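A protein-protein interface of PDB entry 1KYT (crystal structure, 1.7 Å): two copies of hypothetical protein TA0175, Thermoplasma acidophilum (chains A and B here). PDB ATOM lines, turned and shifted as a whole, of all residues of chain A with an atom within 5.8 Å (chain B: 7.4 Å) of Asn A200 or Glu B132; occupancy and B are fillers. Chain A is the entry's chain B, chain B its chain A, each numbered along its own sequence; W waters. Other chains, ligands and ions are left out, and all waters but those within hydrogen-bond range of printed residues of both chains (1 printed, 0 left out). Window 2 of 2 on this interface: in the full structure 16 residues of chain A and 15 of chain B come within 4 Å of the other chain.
OE1 of Glu B132 sits at hydrogen-bond distance from ND2 of Asn A200, 3.0 Å away.
The side-chain hydroxyl of Ser B133 sits close to the backbone carbonyl oxygen of Lys B129, 3.5 Å away. The backbone carbonyl oxygen (O) of Glu B130 lies within hydrogen-bond range of the side-chain hydroxyl (OG) of Ser B133. N of Arg B150 is in hydrogen-bond range of O of Gly B135 (3.2 Å).
Met A182 touches Arg B150 (CE to NH2, 3.7 Å). Asn A200 touches Arg B150 (ND2 to NH2, 3.8 Å). O of Glu B132 touches CB of Ala A203, at 3.6 Å. CB of Ala A203 touches O of Ser B133, at 3.5 Å. Gly B135 touches Ala A203 (N to CB, 3.5 Å). Val A204 touches Gly B135 (CG1 to CA, 3.6 Å). Arg B150 touches Val A204 (CB to CG1, 3.7 Å).
Printed residues of chain B within 4 Å of Met A182: Arg B150 (3.7 Å). Asn A200 touches two residues of chain B. Printed residues of chain B within 4 Å of Val A204: Gly B135 (3.6 Å) and Arg B150 (3.7 Å). Val B127 touches none of the printed residues of chain A. Of the printed residues of chain A, Ser B133 touches Ala A203. Of the printed residues of chain A, Arg B150 touches Met A182, Asn A200 and Val A204. The nearest residue of chain B that does not touch Asn A200 is Ser B133 (4.4 Å). The nearest residue of chain A that does not touch Glu B132 is Asp A199 (5.0 Å).
Printed residues of chain B that touch a printed residue of chain A: Glu B132, Ser B133, Gly B135 and Arg B150. Among the printed residues, 8 pairs touch across the chains. Among the printed residues, no Asp or Glu carboxylate lies within 4 Å of a Lys or Arg side-chain nitrogen of the other chain.
No position is printed for both chains. Of the 8 pairs that touch across the chains among the printed residues, none has its exchanged pair printed and touching as well.
Water W1 bridges O of Asn A200 (2.8 Å) and O of Glu B132 (2.8 Å).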
ATOM      1  N   MET A 182     -39.965  30.406  19.406  1.00  0.00           N
ATOM      2  CA  MET A 182     -38.918  29.463  19.803  1.00  0.00           C
ATOM      3  C   MET A 182     -38.888  29.162  21.301  1.00  0.00           C
ATOM      4  O   MET A 182     -38.582  28.043  21.708  1.00  0.00           O
ATOM      5  CB  MET A 182     -37.536  29.973  19.366  1.00  0.00           C
ATOM      6  CG  MET A 182     -36.384  29.042  19.758  1.00  0.00           C
ATOM      7  SD  MET A 182     -36.624  27.218  19.108  1.00  0.00           S
ATOM      8  CE  MET A 182     -35.784  27.419  17.370  1.00  0.00           C
ATOM      9  N   THR A 198     -40.066  28.754  10.453  1.00  0.00           N
ATOM     10  CA  THR A 198     -38.617  28.892  10.267  1.00  0.00           C
ATOM     11  C   THR A 198     -37.919  27.547  10.190  1.00  0.00           C
ATOM     12  O   THR A 198     -38.448  26.520  10.635  1.00  0.00           O
ATOM     13  CB  THR A 198     -37.941  29.661  11.426  1.00  0.00           C
ATOM     14  OG1 THR A 198     -38.009  28.873  12.621  1.00  0.00           O
ATOM     15  CG2 THR A 198     -38.611  30.994  11.653  1.00  0.00           C
ATOM     16  N   ASP A 199     -36.712  27.554   9.636  1.00  0.00           N
ATOM     17  CA  ASP A 199     -35.940  26.334   9.547  1.00  0.00           C
ATOM     18  C   ASP A 199     -35.595  25.814  10.944  1.00  0.00           C
ATOM     19  O   ASP A 199     -35.620  24.625  11.179  1.00  0.00           O
ATOM     20  CB  ASP A 199     -34.662  26.582   8.744  1.00  0.00           C
ATOM     21  CG  ASP A 199     -34.907  26.560   7.251  1.00  0.00           C
ATOM     22  OD1 ASP A 199     -34.012  26.988   6.489  1.00  0.00           O
ATOM     23  OD2 ASP A 199     -35.993  26.102   6.835  1.00  0.00           O
ATOM     24  N   ASN A 200     -35.282  26.700  11.881  1.00  0.00           N
ATOM     25  CA  ASN A 200     -34.943  26.238  13.223  1.00  0.00           C
ATOM     26  C   ASN A 200     -36.131  25.598  13.959  1.00  0.00           C
ATOM     27  O   ASN A 200     -35.972  24.576  14.645  1.00  0.00           O
ATOM     28  CB  ASN A 200     -34.339  27.394  14.041  1.00  0.00           C
ATOM     29  CG  ASN A 200     -32.862  27.628  13.725  1.00  0.00           C
ATOM     30  OD1 ASN A 200     -32.317  27.028  12.805  1.00  0.00           O
ATOM     31  ND2 ASN A 200     -32.213  28.509  14.490  1.00  0.00           N
ATOM     32  N   ILE A 201     -37.316  26.193  13.826  1.00  0.00           N
ATOM     33  CA  ILE A 201     -38.508  25.642  14.463  1.00  0.00           C
ATOM     34  C   ILE A 201     -38.763  24.251  13.883  1.00  0.00           C
ATOM     35  O   ILE A 201     -38.993  23.297  14.619  1.00  0.00           O
ATOM     36  CB  ILE A 201     -39.777  26.518  14.208  1.00  0.00           C
ATOM     37  CG1 ILE A 201     -39.642  27.884  14.892  1.00  0.00           C
ATOM     38  CG2 ILE A 201     -41.020  25.796  14.728  1.00  0.00           C
ATOM     39  CD1 ILE A 201     -39.526  27.819  16.399  1.00  0.00           C
ATOM     40  N   LYS A 202     -38.716  24.142  12.557  1.00  0.00           N
ATOM     41  CA  LYS A 202     -38.964  22.863  11.902  1.00  0.00           C
ATOM     42  C   LYS A 202     -38.088  21.741  12.423  1.00  0.00           C
ATOM     43  O   LYS A 202     -38.564  20.614  12.628  1.00  0.00           O
ATOM     44  CB  LYS A 202     -38.750  22.988  10.397  1.00  0.00           C
ATOM     45  CG  LYS A 202     -39.764  23.850   9.686  1.00  0.00           C
ATOM     46  CD  LYS A 202     -39.661  23.618   8.191  1.00  0.00           C
ATOM     47  CE  LYS A 202     -40.806  24.264   7.444  1.00  0.00           C
ATOM     48  NZ  LYS A 202     -40.784  23.856   6.011  1.00  0.00           N
ATOM     49  N   ALA A 203     -36.813  22.060  12.640  1.00  0.00           N
ATOM     50  CA  ALA A 203     -35.827  21.087  13.096  1.00  0.00           C
ATOM     51  C   ALA A 203     -36.047  20.570  14.506  1.00  0.00           C
ATOM     52  O   ALA A 203     -35.579  19.487  14.844  1.00  0.00           O
ATOM     53  CB  ALA A 203     -34.436  21.668  12.972  1.00  0.00           C
ATOM     54  N   VAL A 204     -36.748  21.327  15.342  1.00  0.00           N
ATOM     55  CA  VAL A 204     -36.979  20.843  16.691  1.00  0.00           C
ATOM     56  C   VAL A 204     -38.409  20.394  16.916  1.00  0.00           C
ATOM     57  O   VAL A 204     -38.765  19.967  18.010  1.00  0.00           O
ATOM     58  CB  VAL A 204     -36.589  21.896  17.759  1.00  0.00           C
ATOM     59  CG1 VAL A 204     -35.160  22.354  17.514  1.00  0.00           C
ATOM     60  CG2 VAL A 204     -37.558  23.066  17.749  1.00  0.00           C
ATOM     61  N   SER A 205     -39.227  20.468  15.874  1.00  0.00           N
ATOM     62  CA  SER A 205     -40.626  20.056  15.974  1.00  0.00           C
ATOM     63  C   SER A 205     -40.776  18.545  15.822  1.00  0.00           C
ATOM     64  O   SER A 205     -40.030  17.914  15.074  1.00  0.00           O
ATOM     65  CB  SER A 205     -41.461  20.773  14.905  1.00  0.00           C
ATOM     66  OG  SER A 205     -41.565  22.154  15.201  1.00  0.00           O
ATOM     67  N   PHE B  92     -23.355  13.931  14.689  1.00  0.00           N
ATOM     68  CA  PHE B  92     -23.101  15.212  14.047  1.00  0.00           C
ATOM     69  C   PHE B  92     -21.607  15.488  14.119  1.00  0.00           C
ATOM     70  O   PHE B  92     -21.004  15.946  13.155  1.00  0.00           O
ATOM     71  CB  PHE B  92     -23.873  16.322  14.764  1.00  0.00           C
ATOM     72  CG  PHE B  92     -23.712  17.685  14.137  1.00  0.00           C
ATOM     73  CD1 PHE B  92     -24.494  18.067  13.053  1.00  0.00           C
ATOM     74  CD2 PHE B  92     -22.786  18.590  14.644  1.00  0.00           C
ATOM     75  CE1 PHE B  92     -24.356  19.340  12.485  1.00  0.00           C
ATOM     76  CE2 PHE B  92     -22.641  19.867  14.083  1.00  0.00           C
ATOM     77  CZ  PHE B  92     -23.427  20.240  13.004  1.00  0.00           C
ATOM     78  N   TYR B 126     -20.173  28.219  10.366  1.00  0.00           N
ATOM     79  CA  TYR B 126     -20.674  27.117   9.554  1.00  0.00           C
ATOM     80  C   TYR B 126     -21.246  25.978  10.405  1.00  0.00           C
ATOM     81  O   TYR B 126     -22.358  25.503  10.169  1.00  0.00           O
ATOM     82  CB  TYR B 126     -19.553  26.564   8.676  1.00  0.00           C
ATOM     83  CG  TYR B 126     -19.952  25.358   7.852  1.00  0.00           C
ATOM     84  CD1 TYR B 126     -20.870  25.475   6.809  1.00  0.00           C
ATOM     85  CD2 TYR B 126     -19.402  24.101   8.105  1.00  0.00           C
ATOM     86  CE1 TYR B 126     -21.225  24.377   6.037  1.00  0.00           C
ATOM     87  CE2 TYR B 126     -19.758  22.992   7.337  1.00  0.00           C
ATOM     88  CZ  TYR B 126     -20.668  23.143   6.305  1.00  0.00           C
ATOM     89  OH  TYR B 126     -21.028  22.063   5.540  1.00  0.00           O
ATOM     90  N   VAL B 127     -20.483  25.536  11.392  1.00  0.00           N
ATOM     91  CA  VAL B 127     -20.949  24.438  12.241  1.00  0.00           C
ATOM     92  C   VAL B 127     -22.223  24.828  12.993  1.00  0.00           C
ATOM     93  O   VAL B 127     -23.122  24.006  13.172  1.00  0.00           O
ATOM     94  CB  VAL B 127     -19.821  23.969  13.202  1.00  0.00           C
ATOM     95  CG1 VAL B 127     -20.361  23.097  14.298  1.00  0.00           C
ATOM     96  CG2 VAL B 127     -18.790  23.177  12.418  1.00  0.00           C
ATOM     97  N   ARG B 128     -22.331  26.085  13.405  1.00  0.00           N
ATOM     98  CA  ARG B 128     -23.533  26.500  14.125  1.00  0.00           C
ATOM     99  C   ARG B 128     -24.792  26.374  13.251  1.00  0.00           C
ATOM    100  O   ARG B 128     -25.851  25.963  13.736  1.00  0.00           O
ATOM    101  CB  ARG B 128     -23.409  27.933  14.629  1.00  0.00           C
ATOM    102  CG  ARG B 128     -24.692  28.424  15.290  1.00  0.00           C
ATOM    103  CD  ARG B 128     -24.458  29.699  16.071  1.00  0.00           C
ATOM    104  NE  ARG B 128     -23.846  29.440  17.370  1.00  0.00           N
ATOM    105  CZ  ARG B 128     -22.895  30.196  17.900  1.00  0.00           C
ATOM    106  NH1 ARG B 128     -22.453  31.242  17.234  1.00  0.00           N
ATOM    107  NH2 ARG B 128     -22.388  29.906  19.082  1.00  0.00           N
ATOM    108  N   LYS B 129     -24.671  26.740  11.979  1.00  0.00           N
ATOM    109  CA  LYS B 129     -25.784  26.656  11.031  1.00  0.00           C
ATOM    110  C   LYS B 129     -26.149  25.197  10.774  1.00  0.00           C
ATOM    111  O   LYS B 129     -27.322  24.842  10.668  1.00  0.00           O
ATOM    112  CB  LYS B 129     -25.411  27.322   9.705  1.00  0.00           C
ATOM    113  CG  LYS B 129     -25.181  28.820   9.797  1.00  0.00           C
ATOM    114  CD  LYS B 129     -24.924  29.422   8.416  1.00  0.00           C
ATOM    115  CE  LYS B 129     -24.760  30.938   8.485  1.00  0.00           C
ATOM    116  NZ  LYS B 129     -24.615  31.543   7.128  1.00  0.00           N
ATOM    117  N   GLU B 130     -25.142  24.349  10.641  1.00  0.00           N
ATOM    118  CA  GLU B 130     -25.408  22.938  10.428  1.00  0.00           C
ATOM    119  C   GLU B 130     -26.060  22.383  11.701  1.00  0.00           C
ATOM    120  O   GLU B 130     -27.054  21.669  11.643  1.00  0.00           O
ATOM    121  CB  GLU B 130     -24.110  22.196  10.108  1.00  0.00           C
ATOM    122  CG  GLU B 130     -23.552  22.528   8.729  1.00  0.00           C
ATOM    123  CD  GLU B 130     -24.538  22.229   7.606  1.00  0.00           C
ATOM    124  OE1 GLU B 130     -24.687  23.071   6.709  1.00  0.00           O
ATOM    125  OE2 GLU B 130     -25.165  21.154   7.613  1.00  0.00           O
ATOM    126  N   ALA B 131     -25.516  22.751  12.854  1.00  0.00           N
ATOM    127  CA  ALA B 131     -26.054  22.297  14.131  1.00  0.00           C
ATOM    128  C   ALA B 131     -27.527  22.687  14.302  1.00  0.00           C
ATOM    129  O   ALA B 131     -28.364  21.849  14.611  1.00  0.00           O
ATOM    130  CB  ALA B 131     -25.213  22.872  15.288  1.00  0.00           C
ATOM    131  N   GLU B 132     -27.854  23.956  14.093  1.00  0.00           N
ATOM    132  CA  GLU B 132     -29.239  24.387  14.264  1.00  0.00           C
ATOM    133  C   GLU B 132     -30.194  23.734  13.246  1.00  0.00           C
ATOM    134  O   GLU B 132     -31.342  23.435  13.567  1.00  0.00           O
ATOM    135  CB  GLU B 132     -29.332  25.918  14.205  1.00  0.00           C
ATOM    136  CG  GLU B 132     -28.342  26.586  15.120  1.00  0.00           C
ATOM    137  CD  GLU B 132     -28.663  28.039  15.436  1.00  0.00           C
ATOM    138  OE1 GLU B 132     -29.266  28.746  14.588  1.00  0.00           O
ATOM    139  OE2 GLU B 132     -28.291  28.479  16.542  1.00  0.00           O
ATOM    140  N   SER B 133     -29.728  23.517  12.024  1.00  0.00           N
ATOM    141  CA  SER B 133     -30.585  22.881  11.029  1.00  0.00           C
ATOM    142  C   SER B 133     -30.889  21.459  11.485  1.00  0.00           C
ATOM    143  O   SER B 133     -31.757  20.791  10.927  1.00  0.00           O
ATOM    144  CB  SER B 133     -29.890  22.826   9.670  1.00  0.00           C
ATOM    145  OG  SER B 133     -28.848  21.875   9.692  1.00  0.00           O
ATOM    146  N   ARG B 134     -30.167  20.997  12.503  1.00  0.00           N
ATOM    147  CA  ARG B 134     -30.351  19.648  13.014  1.00  0.00           C
ATOM    148  C   ARG B 134     -31.055  19.628  14.369  1.00  0.00           C
ATOM    149  O   ARG B 134     -31.156  18.592  15.008  1.00  0.00           O
ATOM    150  CB  ARG B 134     -28.992  18.955  13.119  1.00  0.00           C
ATOM    151  CG  ARG B 134     -28.242  18.899  11.797  1.00  0.00           C
ATOM    152  CD  ARG B 134     -28.615  17.674  10.981  1.00  0.00           C
ATOM    153  NE  ARG B 134     -27.739  16.543  11.279  1.00  0.00           N
ATOM    154  CZ  ARG B 134     -26.456  16.479  10.929  1.00  0.00           C
ATOM    155  NH1 ARG B 134     -25.894  17.482  10.264  1.00  0.00           N
ATOM    156  NH2 ARG B 134     -25.729  15.414  11.250  1.00  0.00           N
ATOM    157  N   GLY B 135     -31.556  20.776  14.803  1.00  0.00           N
ATOM    158  CA  GLY B 135     -32.227  20.817  16.084  1.00  0.00           C
ATOM    159  C   GLY B 135     -31.267  20.877  17.258  1.00  0.00           C
ATOM    160  O   GLY B 135     -31.653  20.598  18.396  1.00  0.00           O
ATOM    161  N   PHE B 136     -30.013  21.231  16.984  1.00  0.00           N
ATOM    162  CA  PHE B 136     -29.001  21.357  18.037  1.00  0.00           C
ATOM    163  C   PHE B 136     -28.570  22.804  18.119  1.00  0.00           C
ATOM    164  O   PHE B 136     -28.900  23.602  17.246  1.00  0.00           O
ATOM    165  CB  PHE B 136     -27.760  20.514  17.729  1.00  0.00           C
ATOM    166  CG  PHE B 136     -28.053  19.059  17.428  1.00  0.00           C
ATOM    167  CD1 PHE B 136     -28.870  18.303  18.262  1.00  0.00           C
ATOM    168  CD2 PHE B 136     -27.475  18.440  16.322  1.00  0.00           C
ATOM    169  CE1 PHE B 136     -29.107  16.943  17.996  1.00  0.00           C
ATOM    170  CE2 PHE B 136     -27.701  17.085  16.045  1.00  0.00           C
ATOM    171  CZ  PHE B 136     -28.519  16.332  16.889  1.00  0.00           C
ATOM    172  N   VAL B 137     -27.827  23.134  19.174  1.00  0.00           N
ATOM    173  CA  VAL B 137     -27.285  24.479  19.367  1.00  0.00           C
ATOM    174  C   VAL B 137     -25.845  24.304  19.875  1.00  0.00           C
ATOM    175  O   VAL B 137     -25.492  23.239  20.383  1.00  0.00           O
ATOM    176  CB  VAL B 137     -28.067  25.295  20.448  1.00  0.00           C
ATOM    177  CG1 VAL B 137     -29.524  25.503  20.032  1.00  0.00           C
ATOM    178  CG2 VAL B 137     -27.978  24.596  21.768  1.00  0.00           C
ATOM    179  N   ILE B 138     -25.012  25.331  19.731  1.00  0.00           N
ATOM    180  CA  ILE B 138     -23.642  25.241  20.234  1.00  0.00           C
ATOM    181  C   ILE B 138     -23.241  26.520  20.953  1.00  0.00           C
ATOM    182  O   ILE B 138     -23.671  27.614  20.599  1.00  0.00           O
ATOM    183  CB  ILE B 138     -22.580  25.006  19.135  1.00  0.00           C
ATOM    184  CG1 ILE B 138     -22.526  26.206  18.188  1.00  0.00           C
ATOM    185  CG2 ILE B 138     -22.857  23.735  18.377  1.00  0.00           C
ATOM    186  CD1 ILE B 138     -21.354  26.148  17.257  1.00  0.00           C
ATOM    187  N   LEU B 147     -22.186  20.865  22.072  1.00  0.00           N
ATOM    188  CA  LEU B 147     -23.188  20.631  21.044  1.00  0.00           C
ATOM    189  C   LEU B 147     -24.345  20.022  21.797  1.00  0.00           C
ATOM    190  O   LEU B 147     -24.279  18.883  22.292  1.00  0.00           O
ATOM    191  CB  LEU B 147     -22.682  19.646  19.999  1.00  0.00           C
ATOM    192  CG  LEU B 147     -23.707  19.252  18.919  1.00  0.00           C
ATOM    193  CD1 LEU B 147     -24.065  20.473  18.075  1.00  0.00           C
ATOM    194  CD2 LEU B 147     -23.146  18.146  18.051  1.00  0.00           C
ATOM    195  N   ARG B 150     -31.663  21.325  21.547  1.00  0.00           N
ATOM    196  CA  ARG B 150     -32.390  22.555  21.820  1.00  0.00           C
ATOM    197  C   ARG B 150     -33.213  22.390  23.103  1.00  0.00           C
ATOM    198  O   ARG B 150     -33.913  21.394  23.273  1.00  0.00           O
ATOM    199  CB  ARG B 150     -33.307  22.889  20.638  1.00  0.00           C
ATOM    200  CG  ARG B 150     -34.252  24.059  20.865  1.00  0.00           C
ATOM    201  CD  ARG B 150     -33.540  25.414  20.945  1.00  0.00           C
ATOM    202  NE  ARG B 150     -32.985  25.829  19.657  1.00  0.00           N
ATOM    203  CZ  ARG B 150     -32.623  27.070  19.358  1.00  0.00           C
ATOM    204  NH1 ARG B 150     -32.747  28.048  20.252  1.00  0.00           N
ATOM    205  NH2 ARG B 150     -32.134  27.339  18.155  1.00  0.00           N
HETATM  206  O   HOH W   1     -33.290  24.482  15.289  1.00  0.00           O
